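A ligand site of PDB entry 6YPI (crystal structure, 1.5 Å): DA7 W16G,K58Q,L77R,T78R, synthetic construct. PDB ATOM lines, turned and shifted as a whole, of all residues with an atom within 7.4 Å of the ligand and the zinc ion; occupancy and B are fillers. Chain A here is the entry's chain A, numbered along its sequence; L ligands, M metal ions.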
ATOM      1  N   LEU A  14       3.453 -19.156 -12.639  1.00  0.00           N
ATOM      2  CA  LEU A  14       3.246 -20.454 -13.281  1.00  0.00           C
ATOM      3  C   LEU A  14       4.395 -21.409 -12.988  1.00  0.00           C
ATOM      4  O   LEU A  14       4.183 -22.579 -12.664  1.00  0.00           O
ATOM      5  CB  LEU A  14       3.052 -20.289 -14.792  1.00  0.00           C
ATOM      6  CG  LEU A  14       1.752 -19.636 -15.272  1.00  0.00           C
ATOM      7  CD1 LEU A  14       1.759 -19.383 -16.779  1.00  0.00           C
ATOM      8  CD2 LEU A  14       0.554 -20.477 -14.897  1.00  0.00           C
ATOM      9  N   ILE A  17       4.216 -22.548  -9.362  1.00  0.00           N
ATOM     10  CA  ILE A  17       3.161 -23.545  -9.184  1.00  0.00           C
ATOM     11  C   ILE A  17       3.650 -24.916  -9.602  1.00  0.00           C
ATOM     12  O   ILE A  17       3.412 -25.913  -8.905  1.00  0.00           O
ATOM     13  CB  ILE A  17       1.889 -23.122  -9.949  1.00  0.00           C
ATOM     14  CG1 ILE A  17       1.244 -21.914  -9.252  1.00  0.00           C
ATOM     15  CG2 ILE A  17       0.920 -24.305 -10.087  1.00  0.00           C
ATOM     16  CD1 ILE A  17       0.160 -21.215 -10.055  1.00  0.00           C
ATOM     17  N   VAL A  29       0.550 -24.592  -3.521  1.00  0.00           N
ATOM     18  CA  VAL A  29      -0.191 -24.504  -4.784  1.00  0.00           C
ATOM     19  C   VAL A  29      -1.430 -23.639  -4.596  1.00  0.00           C
ATOM     20  O   VAL A  29      -1.746 -22.796  -5.454  1.00  0.00           O
ATOM     21  CB  VAL A  29      -0.536 -25.892  -5.345  1.00  0.00           C
ATOM     22  CG1 VAL A  29      -1.443 -25.716  -6.568  1.00  0.00           C
ATOM     23  CG2 VAL A  29       0.718 -26.663  -5.732  1.00  0.00           C
ATOM     24  N   ARG A  30      -2.149 -23.838  -3.489  1.00  0.00           N
ATOM     25  CA  ARG A  30      -3.367 -23.060  -3.251  1.00  0.00           C
ATOM     26  C   ARG A  30      -3.074 -21.569  -3.266  1.00  0.00           C
ATOM     27  O   ARG A  30      -3.752 -20.789  -3.935  1.00  0.00           O
ATOM     28  CB  ARG A  30      -3.995 -23.453  -1.917  1.00  0.00           C
ATOM     29  CG  ARG A  30      -5.290 -22.720  -1.637  1.00  0.00           C
ATOM     30  CD  ARG A  30      -5.802 -23.030  -0.238  1.00  0.00           C
ATOM     31  NE  ARG A  30      -4.947 -22.455   0.789  1.00  0.00           N
ATOM     32  CZ  ARG A  30      -5.123 -21.244   1.301  1.00  0.00           C
ATOM     33  NH1 ARG A  30      -4.293 -20.795   2.231  1.00  0.00           N
ATOM     34  NH2 ARG A  30      -6.130 -20.483   0.884  1.00  0.00           N
ATOM     35  N   LEU A  32      -0.363 -19.870  -4.317  1.00  0.00           N
ATOM     36  CA  LEU A  32       0.143 -19.385  -5.603  1.00  0.00           C
ATOM     37  C   LEU A  32      -0.974 -19.270  -6.623  1.00  0.00           C
ATOM     38  O   LEU A  32      -0.977 -18.359  -7.454  1.00  0.00           O
ATOM     39  CB  LEU A  32       1.247 -20.306  -6.133  1.00  0.00           C
ATOM     40  CG  LEU A  32       2.568 -20.283  -5.369  1.00  0.00           C
ATOM     41  CD1 LEU A  32       3.382 -21.513  -5.738  1.00  0.00           C
ATOM     42  CD2 LEU A  32       3.329 -19.005  -5.701  1.00  0.00           C
ATOM     43  N   GLN A  33      -1.954 -20.176  -6.573  1.00  0.00           N
ATOM     44  CA  GLN A  33      -3.087 -20.048  -7.492  1.00  0.00           C
ATOM     45  C   GLN A  33      -3.889 -18.799  -7.176  1.00  0.00           C
ATOM     46  O   GLN A  33      -4.386 -18.134  -8.100  1.00  0.00           O
ATOM     47  CB  GLN A  33      -3.982 -21.277  -7.423  1.00  0.00           C
ATOM     48  CG  GLN A  33      -3.442 -22.454  -8.136  1.00  0.00           C
ATOM     49  CD  GLN A  33      -4.427 -23.594  -8.160  1.00  0.00           C
ATOM     50  OE1 GLN A  33      -5.435 -23.581  -7.418  1.00  0.00           O
ATOM     51  NE2 GLN A  33      -4.151 -24.597  -8.968  1.00  0.00           N
ATOM     52  N   LEU A  34      -4.026 -18.459  -5.903  1.00  0.00           N
ATOM     53  CA  LEU A  34      -4.698 -17.227  -5.539  1.00  0.00           C
ATOM     54  C   LEU A  34      -3.942 -16.019  -6.102  1.00  0.00           C
ATOM     55  O   LEU A  34      -4.557 -15.055  -6.568  1.00  0.00           O
ATOM     56  CB  LEU A  34      -4.859 -17.141  -4.015  1.00  0.00           C
ATOM     57  CG  LEU A  34      -5.852 -18.136  -3.387  1.00  0.00           C
ATOM     58  CD1 LEU A  34      -5.719 -18.166  -1.882  1.00  0.00           C
ATOM     59  CD2 LEU A  34      -7.280 -17.761  -3.757  1.00  0.00           C
ATOM     60  N   ASN A  35      -2.603 -16.074  -6.080  1.00  0.00           N
ATOM     61  CA  ASN A  35      -1.831 -14.975  -6.646  1.00  0.00           C
ATOM     62  C   ASN A  35      -2.001 -14.928  -8.155  1.00  0.00           C
ATOM     63  O   ASN A  35      -2.183 -13.841  -8.728  1.00  0.00           O
ATOM     64  CB  ASN A  35      -0.355 -15.116  -6.309  1.00  0.00           C
ATOM     65  CG  ASN A  35      -0.094 -15.086  -4.817  1.00  0.00           C
ATOM     66  OD1 ASN A  35      -0.949 -14.677  -4.037  1.00  0.00           O
ATOM     67  ND2 ASN A  35       1.088 -15.541  -4.410  1.00  0.00           N
ATOM     68  N   LEU A  36      -1.927 -16.082  -8.806  1.00  0.00           N
ATOM     69  CA  LEU A  36      -2.156 -16.148 -10.237  1.00  0.00           C
ATOM     70  C   LEU A  36      -3.517 -15.596 -10.589  1.00  0.00           C
ATOM     71  O   LEU A  36      -3.672 -14.885 -11.604  1.00  0.00           O
ATOM     72  CB  LEU A  36      -2.011 -17.600 -10.704  1.00  0.00           C
ATOM     73  CG  LEU A  36      -2.162 -17.842 -12.193  1.00  0.00           C
ATOM     74  CD1 LEU A  36      -0.998 -17.240 -12.952  1.00  0.00           C
ATOM     75  CD2 LEU A  36      -2.291 -19.342 -12.492  1.00  0.00           C
ATOM     76  N   CYS A  37      -4.533 -15.892  -9.773  1.00  0.00           N
ATOM     77  CA  CYS A  37      -5.870 -15.364 -10.019  1.00  0.00           C
ATOM     78  C   CYS A  37      -5.851 -13.834  -9.978  1.00  0.00           C
ATOM     79  O   CYS A  37      -6.407 -13.183 -10.872  1.00  0.00           O
ATOM     80  CB  CYS A  37      -6.847 -15.919  -8.967  1.00  0.00           C
ATOM     81  SG  CYS A  37      -8.546 -15.339  -9.160  1.00  0.00           S
ATOM     82  N   GLN A  38      -5.231 -13.258  -8.941  1.00  0.00           N
ATOM     83  CA  GLN A  38      -5.083 -11.805  -8.841  1.00  0.00           C
ATOM     84  C   GLN A  38      -4.535 -11.236 -10.130  1.00  0.00           C
ATOM     85  O   GLN A  38      -5.046 -10.235 -10.655  1.00  0.00           O
ATOM     86  CB  GLN A  38      -4.118 -11.446  -7.711  1.00  0.00           C
ATOM     87  CG  GLN A  38      -4.578 -11.742  -6.298  1.00  0.00           C
ATOM     88  CD  GLN A  38      -3.636 -11.099  -5.279  1.00  0.00           C
ATOM     89  OE1 GLN A  38      -2.992 -11.776  -4.481  1.00  0.00           O
ATOM     90  NE2 GLN A  38      -3.561  -9.778  -5.313  1.00  0.00           N
ATOM     91  N   MET A  40      -4.385 -12.677 -13.142  1.00  0.00           N
ATOM     92  CA  MET A  40      -5.235 -12.936 -14.307  1.00  0.00           C
ATOM     93  C   MET A  40      -6.409 -11.984 -14.369  1.00  0.00           C
ATOM     94  O   MET A  40      -6.810 -11.560 -15.465  1.00  0.00           O
ATOM     95  CB  MET A  40      -5.755 -14.376 -14.300  1.00  0.00           C
ATOM     96  CG  MET A  40      -4.722 -15.379 -14.710  1.00  0.00           C
ATOM     97  SD  MET A  40      -5.321 -17.038 -14.466  1.00  0.00           S
ATOM     98  CE  MET A  40      -6.556 -17.063 -15.742  1.00  0.00           C
ATOM     99  N   VAL A  41      -7.007 -11.639 -13.220  1.00  0.00           N
ATOM    100  CA  VAL A  41      -8.144 -10.723 -13.242  1.00  0.00           C
ATOM    101  C   VAL A  41      -7.701  -9.359 -13.750  1.00  0.00           C
ATOM    102  O   VAL A  41      -8.461  -8.658 -14.433  1.00  0.00           O
ATOM    103  CB  VAL A  41      -8.815 -10.676 -11.854  1.00  0.00           C
ATOM    104  CG1 VAL A  41      -9.953  -9.699 -11.850  1.00  0.00           C
ATOM    105  CG2 VAL A  41      -9.332 -12.052 -11.479  1.00  0.00           C
ATOM    106  N   HIS A  63     -11.730 -18.896 -17.353  1.00  0.00           N
ATOM    107  CA  HIS A  63     -11.471 -18.478 -15.966  1.00  0.00           C
ATOM    108  C   HIS A  63     -12.775 -18.130 -15.250  1.00  0.00           C
ATOM    109  O   HIS A  63     -12.984 -18.535 -14.102  1.00  0.00           O
ATOM    110  CB  HIS A  63     -10.524 -17.283 -15.982  1.00  0.00           C
ATOM    111  CG  HIS A  63     -10.206 -16.760 -14.623  1.00  0.00           C
ATOM    112  ND1 HIS A  63     -10.552 -15.488 -14.212  1.00  0.00           N
ATOM    113  CD2 HIS A  63      -9.591 -17.339 -13.569  1.00  0.00           C
ATOM    114  CE1 HIS A  63     -10.143 -15.314 -12.969  1.00  0.00           C
ATOM    115  NE2 HIS A  63      -9.554 -16.423 -12.563  1.00  0.00           N
ATOM    116  N   SER A  64     -13.659 -17.389 -15.926  1.00  0.00           N
ATOM    117  CA  SER A  64     -14.936 -17.043 -15.329  1.00  0.00           C
ATOM    118  C   SER A  64     -15.778 -18.280 -15.046  1.00  0.00           C
ATOM    119  O   SER A  64     -16.370 -18.409 -13.967  1.00  0.00           O
ATOM    120  CB  SER A  64     -15.680 -16.069 -16.257  1.00  0.00           C
ATOM    121  OG  SER A  64     -17.015 -15.864 -15.795  1.00  0.00           O
ATOM    122  N   GLY A  66     -14.801 -21.358 -14.485  1.00  0.00           N
ATOM    123  CA  GLY A  66     -14.292 -22.114 -13.365  1.00  0.00           C
ATOM    124  C   GLY A  66     -14.672 -21.492 -12.031  1.00  0.00           C
ATOM    125  O   GLY A  66     -14.938 -22.210 -11.059  1.00  0.00           O
ATOM    126  N   HIS A  67     -14.691 -20.155 -11.961  1.00  0.00           N
ATOM    127  CA  HIS A  67     -15.098 -19.528 -10.709  1.00  0.00           C
ATOM    128  C   HIS A  67     -16.577 -19.735 -10.442  1.00  0.00           C
ATOM    129  O   HIS A  67     -16.984 -19.895  -9.287  1.00  0.00           O
ATOM    130  CB  HIS A  67     -14.738 -18.041 -10.712  1.00  0.00           C
ATOM    131  CG  HIS A  67     -13.331 -17.784 -10.328  1.00  0.00           C
ATOM    132  ND1 HIS A  67     -12.882 -17.916  -9.025  1.00  0.00           N
ATOM    133  CD2 HIS A  67     -12.242 -17.479 -11.076  1.00  0.00           C
ATOM    134  CE1 HIS A  67     -11.581 -17.662  -8.998  1.00  0.00           C
ATOM    135  NE2 HIS A  67     -11.172 -17.384 -10.225  1.00  0.00           N
ATOM    136  N   ILE A  81     -11.791 -27.760 -15.544  1.00  0.00           N
ATOM    137  CA  ILE A  81     -11.587 -26.395 -16.020  1.00  0.00           C
ATOM    138  C   ILE A  81     -10.205 -25.910 -15.637  1.00  0.00           C
ATOM    139  O   ILE A  81      -9.499 -25.298 -16.442  1.00  0.00           O
ATOM    140  CB  ILE A  81     -12.667 -25.470 -15.421  1.00  0.00           C
ATOM    141  CG1 ILE A  81     -14.050 -25.792 -15.976  1.00  0.00           C
ATOM    142  CG2 ILE A  81     -12.288 -24.001 -15.661  1.00  0.00           C
ATOM    143  CD1 ILE A  81     -15.200 -25.143 -15.111  1.00  0.00           C
ATOM    144  N   GLN A  82      -9.795 -26.188 -14.393  1.00  0.00           N
ATOM    145  CA  GLN A  82      -8.469 -25.785 -13.942  1.00  0.00           C
ATOM    146  C   GLN A  82      -7.392 -26.409 -14.798  1.00  0.00           C
ATOM    147  O   GLN A  82      -6.416 -25.737 -15.170  1.00  0.00           O
ATOM    148  CB  GLN A  82      -8.297 -26.184 -12.466  1.00  0.00           C
ATOM    149  CG  GLN A  82      -6.931 -25.874 -11.887  1.00  0.00           C
ATOM    150  CD  GLN A  82      -6.898 -25.982 -10.371  1.00  0.00           C
ATOM    151  OE1 GLN A  82      -5.990 -26.585  -9.798  1.00  0.00           O
ATOM    152  NE2 GLN A  82      -7.899 -25.389  -9.709  1.00  0.00           N
ATOM    153  N   GLU A  83      -7.535 -27.690 -15.128  1.00  0.00           N
ATOM    154  CA  GLU A  83      -6.556 -28.342 -15.984  1.00  0.00           C
ATOM    155  C   GLU A  83      -6.477 -27.645 -17.337  1.00  0.00           C
ATOM    156  O   GLU A  83      -5.396 -27.331 -17.827  1.00  0.00           O
ATOM    157  CB  GLU A  83      -6.906 -29.816 -16.162  1.00  0.00           C
ATOM    158  CG  GLU A  83      -5.943 -30.553 -17.083  1.00  0.00           C
ATOM    159  CD  GLU A  83      -6.365 -31.975 -17.340  1.00  0.00           C
ATOM    160  OE1 GLU A  83      -7.589 -32.241 -17.333  1.00  0.00           O
ATOM    161  OE2 GLU A  83      -5.480 -32.831 -17.544  1.00  0.00           O
ATOM    162  N   LEU A  85      -7.448 -24.583 -18.069  1.00  0.00           N
ATOM    163  CA  LEU A  85      -6.980 -23.212 -17.930  1.00  0.00           C
ATOM    164  C   LEU A  85      -5.460 -23.156 -17.780  1.00  0.00           C
ATOM    165  O   LEU A  85      -4.813 -22.268 -18.334  1.00  0.00           O
ATOM    166  CB  LEU A  85      -7.658 -22.580 -16.721  1.00  0.00           C
ATOM    167  CG  LEU A  85      -7.520 -21.075 -16.551  1.00  0.00           C
ATOM    168  CD1 LEU A  85      -7.922 -20.305 -17.815  1.00  0.00           C
ATOM    169  CD2 LEU A  85      -8.415 -20.695 -15.400  1.00  0.00           C
ATOM    170  N   TYR A  86      -4.886 -24.102 -17.031  1.00  0.00           N
ATOM    171  CA  TYR A  86      -3.429 -24.174 -16.945  1.00  0.00           C
ATOM    172  C   TYR A  86      -2.807 -24.385 -18.311  1.00  0.00           C
ATOM    173  O   TYR A  86      -1.774 -23.776 -18.617  1.00  0.00           O
ATOM    174  CB  TYR A  86      -3.003 -25.307 -16.023  1.00  0.00           C
ATOM    175  CG  TYR A  86      -2.832 -24.846 -14.626  1.00  0.00           C
ATOM    176  CD1 TYR A  86      -1.924 -23.841 -14.314  1.00  0.00           C
ATOM    177  CD2 TYR A  86      -3.582 -25.412 -13.604  1.00  0.00           C
ATOM    178  CE1 TYR A  86      -1.776 -23.406 -12.998  1.00  0.00           C
ATOM    179  CE2 TYR A  86      -3.451 -24.978 -12.300  1.00  0.00           C
ATOM    180  CZ  TYR A  86      -2.550 -23.985 -11.993  1.00  0.00           C
ATOM    181  OH  TYR A  86      -2.423 -23.571 -10.681  1.00  0.00           O
ATOM    182  N   MET A  89      -3.021 -21.157 -20.310  1.00  0.00           N
ATOM    183  CA  MET A  89      -2.091 -20.163 -19.793  1.00  0.00           C
ATOM    184  C   MET A  89      -0.659 -20.487 -20.184  1.00  0.00           C
ATOM    185  O   MET A  89       0.136 -19.587 -20.486  1.00  0.00           O
ATOM    186  CB  MET A  89      -2.202 -20.073 -18.268  1.00  0.00           C
ATOM    187  CG  MET A  89      -3.463 -19.378 -17.762  1.00  0.00           C
ATOM    188  SD  MET A  89      -3.455 -17.587 -17.961  1.00  0.00           S
ATOM    189  CE  MET A  89      -2.323 -17.117 -16.652  1.00  0.00           C
HETATM  190  C1  LIG L   1      -7.689 -19.324 -10.459  1.00  0.00           C
HETATM  191  O1  LIG L   1      -8.024 -19.537  -9.275  1.00  0.00           O
HETATM  192  O2  LIG L   1      -8.092 -18.285 -11.001  1.00  0.00           O
HETATM  193  C2  LIG L   1      -6.830 -20.285 -11.226  1.00  0.00           C
HETATM  194  C3  LIG L   1      -6.389 -19.935 -12.489  1.00  0.00           C
HETATM  195  C4  LIG L   1      -5.604 -20.810 -13.222  1.00  0.00           C
HETATM  196  C5  LIG L   1      -5.254 -22.035 -12.700  1.00  0.00           C
HETATM  197  C6  LIG L   1      -5.679 -22.393 -11.424  1.00  0.00           C
HETATM  198  C7  LIG L   1      -6.478 -21.519 -10.690  1.00  0.00           C
HETATM  199 ZN    ZN M   1      -9.296 -16.816 -10.621  1.00  0.00          ZN
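The zinc ion is bound by O2 of the ligand (1.9 Å), NE2 of His 63 (2.0 Å), NE2 of His 67 (2.0 Å) and SG of Cys 37 (2.2 Å). The zinc ion has four donor atoms within binding distance.
Gln 33 touches the ligand. Leu 36 touches the ligand (CD2 to C4, 3.7 Å). Met 40 touches the ligand. Gln 82 touches the ligand (CG to C6, 3.7 Å). CD2 of Leu 85 touches C4 of the ligand, at 3.6 Å. CZ of Tyr 86 touches C5 of the ligand (3.4 Å).
NE2 of Gln 33 lies within hydrogen-bond range of OH of Tyr 86. NE2 of Gln 33 sits at hydrogen-bond distance from OE1 of Gln 82, 2.8 Å away.
Within 4 Å of the zinc ion: Cys 37, His 63 and His 67. Along chain A the residues within 4 Å of the zinc ion span positions 37 to 67. The nearest printed residue that does not touch the zinc ion is Val 41 (4.8 Å).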
